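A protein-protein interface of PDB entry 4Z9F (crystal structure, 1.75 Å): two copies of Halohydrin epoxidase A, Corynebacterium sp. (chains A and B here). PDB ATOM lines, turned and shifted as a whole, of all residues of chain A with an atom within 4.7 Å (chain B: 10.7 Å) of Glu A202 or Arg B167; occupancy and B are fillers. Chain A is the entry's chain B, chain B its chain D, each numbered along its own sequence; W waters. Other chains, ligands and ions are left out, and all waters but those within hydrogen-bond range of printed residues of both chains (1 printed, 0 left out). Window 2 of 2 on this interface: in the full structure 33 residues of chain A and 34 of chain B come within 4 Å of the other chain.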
ATOM      1  N   ARG A 198      27.369 -27.933 -20.515  1.00  0.00           N
ATOM      2  CA  ARG A 198      26.231 -27.658 -21.386  1.00  0.00           C
ATOM      3  C   ARG A 198      25.302 -26.635 -20.754  1.00  0.00           C
ATOM      4  O   ARG A 198      24.697 -25.817 -21.459  1.00  0.00           O
ATOM      5  CB  ARG A 198      25.488 -28.954 -21.701  1.00  0.00           C
ATOM      6  CG  ARG A 198      26.401 -30.020 -22.281  1.00  0.00           C
ATOM      7  CD  ARG A 198      25.626 -31.150 -22.929  1.00  0.00           C
ATOM      8  NE  ARG A 198      24.785 -31.868 -21.974  1.00  0.00           N
ATOM      9  CZ  ARG A 198      25.209 -32.841 -21.170  1.00  0.00           C
ATOM     10  NH1 ARG A 198      24.353 -33.427 -20.343  1.00  0.00           N
ATOM     11  NH2 ARG A 198      26.482 -33.226 -21.181  1.00  0.00           N
ATOM     12  N   GLU A 199      25.203 -26.649 -19.429  1.00  0.00           N
ATOM     13  CA  GLU A 199      24.379 -25.677 -18.725  1.00  0.00           C
ATOM     14  C   GLU A 199      25.015 -24.291 -18.752  1.00  0.00           C
ATOM     15  O   GLU A 199      24.331 -23.292 -19.008  1.00  0.00           O
ATOM     16  CB  GLU A 199      24.163 -26.174 -17.294  1.00  0.00           C
ATOM     17  CG  GLU A 199      23.836 -25.133 -16.267  1.00  0.00           C
ATOM     18  CD  GLU A 199      23.683 -25.758 -14.894  1.00  0.00           C
ATOM     19  OE1 GLU A 199      24.686 -25.799 -14.144  1.00  0.00           O
ATOM     20  OE2 GLU A 199      22.569 -26.235 -14.579  1.00  0.00           O
ATOM     21  N   ARG A 200      26.325 -24.213 -18.496  1.00  0.00           N
ATOM     22  CA  ARG A 200      27.028 -22.936 -18.573  1.00  0.00           C
ATOM     23  C   ARG A 200      26.990 -22.371 -19.989  1.00  0.00           C
ATOM     24  O   ARG A 200      26.826 -21.160 -20.178  1.00  0.00           O
ATOM     25  CB  ARG A 200      28.473 -23.109 -18.106  1.00  0.00           C
ATOM     26  CG  ARG A 200      29.289 -21.820 -17.989  1.00  0.00           C
ATOM     27  CD  ARG A 200      30.779 -22.127 -18.124  1.00  0.00           C
ATOM     28  NE  ARG A 200      31.041 -23.529 -17.812  1.00  0.00           N
ATOM     29  CZ  ARG A 200      32.184 -24.165 -18.055  1.00  0.00           C
ATOM     30  NH1 ARG A 200      32.298 -25.455 -17.738  1.00  0.00           N
ATOM     31  NH2 ARG A 200      33.212 -23.525 -18.609  1.00  0.00           N
ATOM     32  N   VAL A 201      27.145 -23.229 -20.999  1.00  0.00           N
ATOM     33  CA  VAL A 201      27.085 -22.739 -22.375  1.00  0.00           C
ATOM     34  C   VAL A 201      25.691 -22.214 -22.683  1.00  0.00           C
ATOM     35  O   VAL A 201      25.528 -21.156 -23.308  1.00  0.00           O
ATOM     36  CB  VAL A 201      27.515 -23.844 -23.353  1.00  0.00           C
ATOM     37  CG1 VAL A 201      27.076 -23.499 -24.781  1.00  0.00           C
ATOM     38  CG2 VAL A 201      29.017 -24.042 -23.270  1.00  0.00           C
ATOM     39  N   GLU A 202      24.661 -22.921 -22.212  1.00  0.00           N
ATOM     40  CA  GLU A 202      23.293 -22.473 -22.444  1.00  0.00           C
ATOM     41  C   GLU A 202      23.059 -21.098 -21.831  1.00  0.00           C
ATOM     42  O   GLU A 202      22.373 -20.256 -22.419  1.00  0.00           O
ATOM     43  CB  GLU A 202      22.312 -23.508 -21.883  1.00  0.00           C
ATOM     44  CG  GLU A 202      20.851 -23.358 -22.345  1.00  0.00           C
ATOM     45  CD  GLU A 202      20.143 -22.185 -21.678  1.00  0.00           C
ATOM     46  OE1 GLU A 202      19.310 -21.539 -22.352  1.00  0.00           O
ATOM     47  OE2 GLU A 202      20.452 -21.887 -20.496  1.00  0.00           O
ATOM     48  N   ARG A 203      23.651 -20.838 -20.670  1.00  0.00           N
ATOM     49  CA  ARG A 203      23.405 -19.571 -19.990  1.00  0.00           C
ATOM     50  C   ARG A 203      24.296 -18.442 -20.515  1.00  0.00           C
ATOM     51  O   ARG A 203      23.829 -17.307 -20.664  1.00  0.00           O
ATOM     52  CB  ARG A 203      23.607 -19.757 -18.491  1.00  0.00           C
ATOM     53  CG  ARG A 203      23.639 -18.479 -17.675  1.00  0.00           C
ATOM     54  CD  ARG A 203      24.554 -18.675 -16.480  1.00  0.00           C
ATOM     55  NE  ARG A 203      24.614 -20.083 -16.085  1.00  0.00           N
ATOM     56  CZ  ARG A 203      25.701 -20.684 -15.608  1.00  0.00           C
ATOM     57  NH1 ARG A 203      26.834 -19.997 -15.468  1.00  0.00           N
ATOM     58  NH2 ARG A 203      25.660 -21.972 -15.280  1.00  0.00           N
ATOM     59  N   ASP A 204      25.570 -18.725 -20.804  1.00  0.00           N
ATOM     60  CA  ASP A 204      26.553 -17.672 -21.040  1.00  0.00           C
ATOM     61  C   ASP A 204      26.916 -17.449 -22.503  1.00  0.00           C
ATOM     62  O   ASP A 204      27.495 -16.402 -22.821  1.00  0.00           O
ATOM     63  CB  ASP A 204      27.845 -17.968 -20.272  1.00  0.00           C
ATOM     64  CG  ASP A 204      27.658 -17.889 -18.774  1.00  0.00           C
ATOM     65  OD1 ASP A 204      26.648 -17.305 -18.336  1.00  0.00           O
ATOM     66  OD2 ASP A 204      28.522 -18.410 -18.040  1.00  0.00           O
ATOM     67  N   VAL A 205      26.612 -18.389 -23.389  1.00  0.00           N
ATOM     68  CA  VAL A 205      27.029 -18.334 -24.785  1.00  0.00           C
ATOM     69  C   VAL A 205      25.785 -18.087 -25.636  1.00  0.00           C
ATOM     70  O   VAL A 205      24.976 -19.006 -25.818  1.00  0.00           O
ATOM     71  CB  VAL A 205      27.742 -19.625 -25.216  1.00  0.00           C
ATOM     72  CG1 VAL A 205      28.265 -19.494 -26.644  1.00  0.00           C
ATOM     73  CG2 VAL A 205      28.856 -19.963 -24.231  1.00  0.00           C
ATOM     74  N   PRO A 206      25.609 -16.887 -26.192  1.00  0.00           N
ATOM     75  CA  PRO A 206      24.438 -16.627 -27.056  1.00  0.00           C
ATOM     76  C   PRO A 206      24.267 -17.604 -28.213  1.00  0.00           C
ATOM     77  O   PRO A 206      23.130 -17.912 -28.579  1.00  0.00           O
ATOM     78  CB  PRO A 206      24.704 -15.204 -27.561  1.00  0.00           C
ATOM     79  CG  PRO A 206      25.485 -14.564 -26.437  1.00  0.00           C
ATOM     80  CD  PRO A 206      26.376 -15.659 -25.895  1.00  0.00           C
ATOM     81  N   LEU A 207      25.355 -18.078 -28.826  1.00  0.00           N
ATOM     82  CA  LEU A 207      25.208 -19.058 -29.901  1.00  0.00           C
ATOM     83  C   LEU A 207      24.565 -20.344 -29.404  1.00  0.00           C
ATOM     84  O   LEU A 207      23.942 -21.076 -30.187  1.00  0.00           O
ATOM     85  CB  LEU A 207      26.566 -19.378 -30.521  1.00  0.00           C
ATOM     86  CG  LEU A 207      26.870 -18.869 -31.918  1.00  0.00           C
ATOM     87  CD1 LEU A 207      28.015 -19.681 -32.551  1.00  0.00           C
ATOM     88  CD2 LEU A 207      25.622 -18.846 -32.822  1.00  0.00           C
ATOM     89  N   GLY A 208      24.725 -20.646 -28.127  1.00  0.00           N
ATOM     90  CA  GLY A 208      24.133 -21.828 -27.542  1.00  0.00           C
ATOM     91  C   GLY A 208      24.900 -23.104 -27.798  1.00  0.00           C
ATOM     92  O   GLY A 208      24.365 -24.190 -27.546  1.00  0.00           O
ATOM     93  N   ILE B 118      13.278  -9.222 -37.002  1.00  0.00           N
ATOM     94  CA  ILE B 118      13.531 -10.361 -36.122  1.00  0.00           C
ATOM     95  C   ILE B 118      12.554 -11.496 -36.412  1.00  0.00           C
ATOM     96  O   ILE B 118      12.967 -12.631 -36.669  1.00  0.00           O
ATOM     97  CB  ILE B 118      13.484  -9.923 -34.650  1.00  0.00           C
ATOM     98  CG1 ILE B 118      14.623  -8.938 -34.365  1.00  0.00           C
ATOM     99  CG2 ILE B 118      13.580 -11.115 -33.746  1.00  0.00           C
ATOM    100  CD1 ILE B 118      14.459  -8.173 -33.090  1.00  0.00           C
ATOM    101  N   LEU B 121      13.110 -13.161 -39.974  1.00  0.00           N
ATOM    102  CA  LEU B 121      14.410 -13.821 -40.036  1.00  0.00           C
ATOM    103  C   LEU B 121      14.433 -15.052 -39.137  1.00  0.00           C
ATOM    104  O   LEU B 121      15.022 -16.078 -39.495  1.00  0.00           O
ATOM    105  CB  LEU B 121      15.542 -12.853 -39.656  1.00  0.00           C
ATOM    106  CG  LEU B 121      15.763 -11.607 -40.528  1.00  0.00           C
ATOM    107  CD1 LEU B 121      17.013 -10.824 -40.118  1.00  0.00           C
ATOM    108  CD2 LEU B 121      15.788 -11.943 -42.018  1.00  0.00           C
ATOM    109  N   ARG B 122      13.811 -14.963 -37.958  1.00  0.00           N
ATOM    110  CA  ARG B 122      13.762 -16.109 -37.057  1.00  0.00           C
ATOM    111  C   ARG B 122      12.927 -17.233 -37.653  1.00  0.00           C
ATOM    112  O   ARG B 122      13.328 -18.403 -37.616  1.00  0.00           O
ATOM    113  CB  ARG B 122      13.205 -15.706 -35.691  1.00  0.00           C
ATOM    114  CG  ARG B 122      12.720 -16.906 -34.892  1.00  0.00           C
ATOM    115  CD  ARG B 122      12.671 -16.631 -33.409  1.00  0.00           C
ATOM    116  NE  ARG B 122      11.736 -15.569 -33.097  1.00  0.00           N
ATOM    117  CZ  ARG B 122      12.054 -14.456 -32.448  1.00  0.00           C
ATOM    118  NH1 ARG B 122      11.122 -13.551 -32.218  1.00  0.00           N
ATOM    119  NH2 ARG B 122      13.292 -14.252 -32.020  1.00  0.00           N
ATOM    120  N   ALA B 123      11.757 -16.893 -38.196  1.00  0.00           N
ATOM    121  CA  ALA B 123      10.922 -17.889 -38.859  1.00  0.00           C
ATOM    122  C   ALA B 123      11.711 -18.662 -39.905  1.00  0.00           C
ATOM    123  O   ALA B 123      11.592 -19.888 -40.005  1.00  0.00           O
ATOM    124  CB  ALA B 123       9.708 -17.210 -39.498  1.00  0.00           C
ATOM    125  N   ALA B 124      12.545 -17.967 -40.676  1.00  0.00           N
ATOM    126  CA  ALA B 124      13.258 -18.608 -41.772  1.00  0.00           C
ATOM    127  C   ALA B 124      14.464 -19.420 -41.316  1.00  0.00           C
ATOM    128  O   ALA B 124      15.094 -20.080 -42.147  1.00  0.00           O
ATOM    129  CB  ALA B 124      13.698 -17.558 -42.796  1.00  0.00           C
ATOM    130  N   GLY B 125      14.805 -19.393 -40.036  1.00  0.00           N
ATOM    131  CA  GLY B 125      15.907 -20.184 -39.531  1.00  0.00           C
ATOM    132  C   GLY B 125      17.216 -19.447 -39.391  1.00  0.00           C
ATOM    133  O   GLY B 125      18.269 -20.094 -39.345  1.00  0.00           O
ATOM    134  N   GLY B 126      17.187 -18.127 -39.342  1.00  0.00           N
ATOM    135  CA  GLY B 126      18.378 -17.338 -39.116  1.00  0.00           C
ATOM    136  C   GLY B 126      18.721 -16.469 -40.310  1.00  0.00           C
ATOM    137  O   GLY B 126      18.106 -16.538 -41.371  1.00  0.00           O
ATOM    138  N   ALA B 127      19.755 -15.652 -40.099  1.00  0.00           N
ATOM    139  CA  ALA B 127      20.220 -14.674 -41.070  1.00  0.00           C
ATOM    140  C   ALA B 127      21.419 -13.936 -40.500  1.00  0.00           C
ATOM    141  O   ALA B 127      21.783 -14.135 -39.337  1.00  0.00           O
ATOM    142  CB  ALA B 127      19.112 -13.674 -41.422  1.00  0.00           C
ATOM    143  N   SER B 160      24.543  -5.771 -27.619  1.00  0.00           N
ATOM    144  CA  SER B 160      23.508  -6.216 -26.691  1.00  0.00           C
ATOM    145  C   SER B 160      22.487  -7.118 -27.379  1.00  0.00           C
ATOM    146  O   SER B 160      22.137  -8.179 -26.851  1.00  0.00           O
ATOM    147  CB  SER B 160      22.812  -5.008 -26.055  1.00  0.00           C
ATOM    148  OG  SER B 160      21.721  -5.443 -25.270  1.00  0.00           O
ATOM    149  N   ALA B 161      21.992  -6.711 -28.550  1.00  0.00           N
ATOM    150  CA  ALA B 161      20.953  -7.501 -29.208  1.00  0.00           C
ATOM    151  C   ALA B 161      21.457  -8.888 -29.578  1.00  0.00           C
ATOM    152  O   ALA B 161      20.685  -9.849 -29.564  1.00  0.00           O
ATOM    153  CB  ALA B 161      20.437  -6.796 -30.459  1.00  0.00           C
ATOM    154  N   ALA B 162      22.745  -9.012 -29.902  1.00  0.00           N
ATOM    155  CA  ALA B 162      23.300 -10.317 -30.246  1.00  0.00           C
ATOM    156  C   ALA B 162      23.223 -11.314 -29.094  1.00  0.00           C
ATOM    157  O   ALA B 162      23.280 -12.524 -29.334  1.00  0.00           O
ATOM    158  CB  ALA B 162      24.757 -10.167 -30.681  1.00  0.00           C
ATOM    159  N   LYS B 163      23.131 -10.843 -27.851  1.00  0.00           N
ATOM    160  CA  LYS B 163      23.083 -11.770 -26.729  1.00  0.00           C
ATOM    161  C   LYS B 163      21.827 -12.628 -26.770  1.00  0.00           C
ATOM    162  O   LYS B 163      21.840 -13.758 -26.275  1.00  0.00           O
ATOM    163  CB  LYS B 163      23.161 -11.013 -25.397  1.00  0.00           C
ATOM    164  CG  LYS B 163      24.340 -10.052 -25.263  1.00  0.00           C
ATOM    165  CD  LYS B 163      25.689 -10.743 -25.479  1.00  0.00           C
ATOM    166  CE  LYS B 163      26.842  -9.822 -25.036  1.00  0.00           C
ATOM    167  NZ  LYS B 163      28.195 -10.314 -25.477  1.00  0.00           N
ATOM    168  N   THR B 164      20.742 -12.117 -27.350  1.00  0.00           N
ATOM    169  CA  THR B 164      19.505 -12.877 -27.482  1.00  0.00           C
ATOM    170  C   THR B 164      19.247 -13.383 -28.902  1.00  0.00           C
ATOM    171  O   THR B 164      18.790 -14.517 -29.070  1.00  0.00           O
ATOM    172  CB  THR B 164      18.311 -12.037 -27.001  1.00  0.00           C
ATOM    173  OG1 THR B 164      18.286 -10.779 -27.682  1.00  0.00           O
ATOM    174  CG2 THR B 164      18.414 -11.789 -25.513  1.00  0.00           C
ATOM    175  N   LEU B 165      19.553 -12.595 -29.939  1.00  0.00           N
ATOM    176  CA  LEU B 165      19.220 -13.029 -31.297  1.00  0.00           C
ATOM    177  C   LEU B 165      20.111 -14.167 -31.801  1.00  0.00           C
ATOM    178  O   LEU B 165      19.680 -14.925 -32.679  1.00  0.00           O
ATOM    179  CB  LEU B 165      19.298 -11.846 -32.260  1.00  0.00           C
ATOM    180  CG  LEU B 165      18.306 -10.715 -32.000  1.00  0.00           C
ATOM    181  CD1 LEU B 165      18.471  -9.615 -33.051  1.00  0.00           C
ATOM    182  CD2 LEU B 165      16.871 -11.249 -31.972  1.00  0.00           C
ATOM    183  N   SER B 166      21.326 -14.317 -31.261  1.00  0.00           N
ATOM    184  CA  SER B 166      22.234 -15.363 -31.736  1.00  0.00           C
ATOM    185  C   SER B 166      21.642 -16.761 -31.565  1.00  0.00           C
ATOM    186  O   SER B 166      21.936 -17.653 -32.368  1.00  0.00           O
ATOM    187  CB  SER B 166      23.581 -15.275 -31.006  1.00  0.00           C
ATOM    188  OG  SER B 166      24.255 -14.048 -31.275  1.00  0.00           O
ATOM    189  N   ARG B 167      20.809 -16.974 -30.537  1.00  0.00           N
ATOM    190  CA  ARG B 167      20.173 -18.283 -30.361  1.00  0.00           C
ATOM    191  C   ARG B 167      19.161 -18.595 -31.451  1.00  0.00           C
ATOM    192  O   ARG B 167      18.873 -19.774 -31.685  1.00  0.00           O
ATOM    193  CB  ARG B 167      19.470 -18.397 -29.006  1.00  0.00           C
ATOM    194  CG  ARG B 167      20.393 -18.474 -27.860  1.00  0.00           C
ATOM    195  CD  ARG B 167      20.947 -19.878 -27.713  1.00  0.00           C
ATOM    196  NE  ARG B 167      20.524 -20.453 -26.448  1.00  0.00           N
ATOM    197  CZ  ARG B 167      21.181 -20.284 -25.306  1.00  0.00           C
ATOM    198  NH1 ARG B 167      22.293 -19.552 -25.259  1.00  0.00           N
ATOM    199  NH2 ARG B 167      20.722 -20.831 -24.185  1.00  0.00           N
ATOM    200  N   ASP B 168      18.600 -17.575 -32.100  1.00  0.00           N
ATOM    201  CA  ASP B 168      17.662 -17.758 -33.198  1.00  0.00           C
ATOM    202  C   ASP B 168      18.352 -17.927 -34.549  1.00  0.00           C
ATOM    203  O   ASP B 168      17.673 -17.949 -35.576  1.00  0.00           O
ATOM    204  CB  ASP B 168      16.695 -16.571 -33.281  1.00  0.00           C
ATOM    205  CG  ASP B 168      15.838 -16.401 -32.034  1.00  0.00           C
ATOM    206  OD1 ASP B 168      15.369 -17.410 -31.469  1.00  0.00           O
ATOM    207  OD2 ASP B 168      15.631 -15.235 -31.623  1.00  0.00           O
ATOM    208  N   GLY B 169      19.676 -18.048 -34.579  1.00  0.00           N
ATOM    209  CA  GLY B 169      20.387 -18.043 -35.840  1.00  0.00           C
ATOM    210  C   GLY B 169      20.521 -16.682 -36.498  1.00  0.00           C
ATOM    211  O   GLY B 169      20.976 -16.608 -37.645  1.00  0.00           O
ATOM    212  N   ILE B 170      20.134 -15.608 -35.817  1.00  0.00           N
ATOM    213  CA  ILE B 170      20.194 -14.251 -36.363  1.00  0.00           C
ATOM    214  C   ILE B 170      21.491 -13.624 -35.860  1.00  0.00           C
ATOM    215  O   ILE B 170      21.582 -13.234 -34.693  1.00  0.00           O
ATOM    216  CB  ILE B 170      18.984 -13.419 -35.935  1.00  0.00           C
ATOM    217  CG1 ILE B 170      17.671 -14.116 -36.325  1.00  0.00           C
ATOM    218  CG2 ILE B 170      19.056 -12.040 -36.556  1.00  0.00           C
ATOM    219  CD1 ILE B 170      16.458 -13.520 -35.624  1.00  0.00           C
ATOM    220  N   LEU B 171      22.495 -13.521 -36.730  1.00  0.00           N
ATOM    221  CA  LEU B 171      23.853 -13.171 -36.316  1.00  0.00           C
ATOM    222  C   LEU B 171      24.131 -11.704 -36.630  1.00  0.00           C
ATOM    223  O   LEU B 171      24.122 -11.312 -37.797  1.00  0.00           O
ATOM    224  CB  LEU B 171      24.867 -14.082 -37.013  1.00  0.00           C
ATOM    225  CG  LEU B 171      24.542 -15.581 -36.913  1.00  0.00           C
ATOM    226  CD1 LEU B 171      25.550 -16.385 -37.704  1.00  0.00           C
ATOM    227  CD2 LEU B 171      24.477 -16.059 -35.450  1.00  0.00           C
ATOM    228  N   LEU B 172      24.411 -10.902 -35.592  1.00  0.00           N
ATOM    229  CA  LEU B 172      24.612  -9.462 -35.752  1.00  0.00           C
ATOM    230  C   LEU B 172      26.091  -9.096 -35.686  1.00  0.00           C
ATOM    231  O   LEU B 172      26.844  -9.634 -34.872  1.00  0.00           O
ATOM    232  CB  LEU B 172      23.846  -8.679 -34.678  1.00  0.00           C
ATOM    233  CG  LEU B 172      22.420  -8.253 -35.041  1.00  0.00           C
ATOM    234  CD1 LEU B 172      21.553  -9.458 -35.395  1.00  0.00           C
ATOM    235  CD2 LEU B 172      21.795  -7.463 -33.912  1.00  0.00           C
ATOM    236  N   ARG B 226      28.205 -17.056 -42.893  1.00  0.00           N
ATOM    237  CA  ARG B 226      28.022 -17.697 -41.592  1.00  0.00           C
ATOM    238  C   ARG B 226      29.059 -18.787 -41.307  1.00  0.00           C
ATOM    239  O   ARG B 226      28.926 -19.517 -40.314  1.00  0.00           O
ATOM    240  CB  ARG B 226      26.597 -18.269 -41.442  1.00  0.00           C
ATOM    241  CG  ARG B 226      25.509 -17.223 -41.665  1.00  0.00           C
ATOM    242  CD  ARG B 226      24.124 -17.691 -41.232  1.00  0.00           C
ATOM    243  NE  ARG B 226      23.138 -17.381 -42.263  1.00  0.00           N
ATOM    244  CZ  ARG B 226      21.896 -17.856 -42.307  1.00  0.00           C
ATOM    245  NH1 ARG B 226      21.443 -18.681 -41.363  1.00  0.00           N
ATOM    246  NH2 ARG B 226      21.104 -17.491 -43.306  1.00  0.00           N
ATOM    247  N   ALA B 229      30.505 -18.382 -37.597  1.00  0.00           N
ATOM    248  CA  ALA B 229      29.473 -17.905 -36.678  1.00  0.00           C
ATOM    249  C   ALA B 229      29.976 -17.468 -35.299  1.00  0.00           C
ATOM    250  O   ALA B 229      29.443 -16.478 -34.769  1.00  0.00           O
ATOM    251  CB  ALA B 229      28.408 -19.001 -36.524  1.00  0.00           C
ATOM    252  N   VAL B 232      30.227 -13.842 -33.857  1.00  0.00           N
ATOM    253  CA  VAL B 232      29.010 -13.030 -33.839  1.00  0.00           C
ATOM    254  C   VAL B 232      29.045 -12.011 -32.695  1.00  0.00           C
ATOM    255  O   VAL B 232      29.645 -12.238 -31.637  1.00  0.00           O
ATOM    256  CB  VAL B 232      27.774 -13.943 -33.718  1.00  0.00           C
ATOM    257  CG1 VAL B 232      27.827 -14.747 -32.420  1.00  0.00           C
ATOM    258  CG2 VAL B 232      26.468 -13.151 -33.765  1.00  0.00           C
ATOM    259  N   GLY B 233      28.409 -10.864 -32.917  1.00  0.00           N
ATOM    260  CA  GLY B 233      28.104  -9.956 -31.828  1.00  0.00           C
ATOM    261  C   GLY B 233      29.183  -8.973 -31.441  1.00  0.00           C
ATOM    262  O   GLY B 233      29.176  -8.490 -30.302  1.00  0.00           O
HETATM  263  O   HOH W   1      22.307 -20.292 -32.470  1.00  0.00           O
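Among the printed residues, merely in contact across the chains: Pro A206 with Lys B163, Pro A206 with Ala B162, Pro A206 with Ser B166, Gly A208 with Arg B167, Leu A207 with Ser B166 and Leu A207 with Leu B171.
Hydrophobic or aromatic side chains of chain B within 4 Å of the printed part of chain A: Leu B171. Of the 11 printed residues of chain A, 5 touch a printed residue of chain B. Hydrophobic or aromatic side chains of chain A within 4 Å of the printed part of chain B: Pro A206 and Leu A207.
Water W1 lies within hydrogen-bond range of O of Ser B166 (2.7 Å) and O of Leu A207 (2.9 Å).
The side-chain carboxylate of Glu A202 is in salt-bridge range of the guanidinium group of Arg B167, at 2.4 Å. The backbone carbonyl oxygen (O) of Val A205 lies within hydrogen-bond range of the guanidinium group (NH1) of Arg B167 (2.8 Å). N of Arg B167 lies close to O of Pro A206.
Val A201 touches none of the printed residues of chain B. Glu A202 touches just one residue of chain B: Arg B167. Val A205 touches just one residue of chain B: Arg B167 (2.8 Å). Printed residues of chain B within 4 Å of Leu A207: Ser B166 and Leu B171. Of the printed residues of chain A, Ala B162 touches Pro A206. Of the printed residues of chain A, Lys B163 touches Pro A206 (3.5 Å). Leu B165 touches none of the printed residues of chain A. Of the printed residues of chain A, Ser B166 touches Pro A206 and Leu A207. Of chain A, only Glu A202 (2.4 Å), Val A205 (2.8 Å), Pro A206 (2.9 Å) and Gly A208 (3.7 Å) come within 4 Å of Arg B167. Printed residues of chain A within 4 Å of Leu B171: Leu A207. The nearest residue of chain A that does not touch Arg B167 is Leu A207 (4.02 Å).
No position is printed for both chains. Of the 9 pairs that touch across the chains among the printed residues, none has its exchanged pair printed and touching as well.
The backbone NH of Leu B171 sits at hydrogen-bond distance from the backbone carbonyl oxygen of Ala B127. The backbone carbonyl oxygen (O) of Ala B162 lies within hydrogen-bond range of the side-chain hydroxyl (OG) of Ser B166 (2.7 Å).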
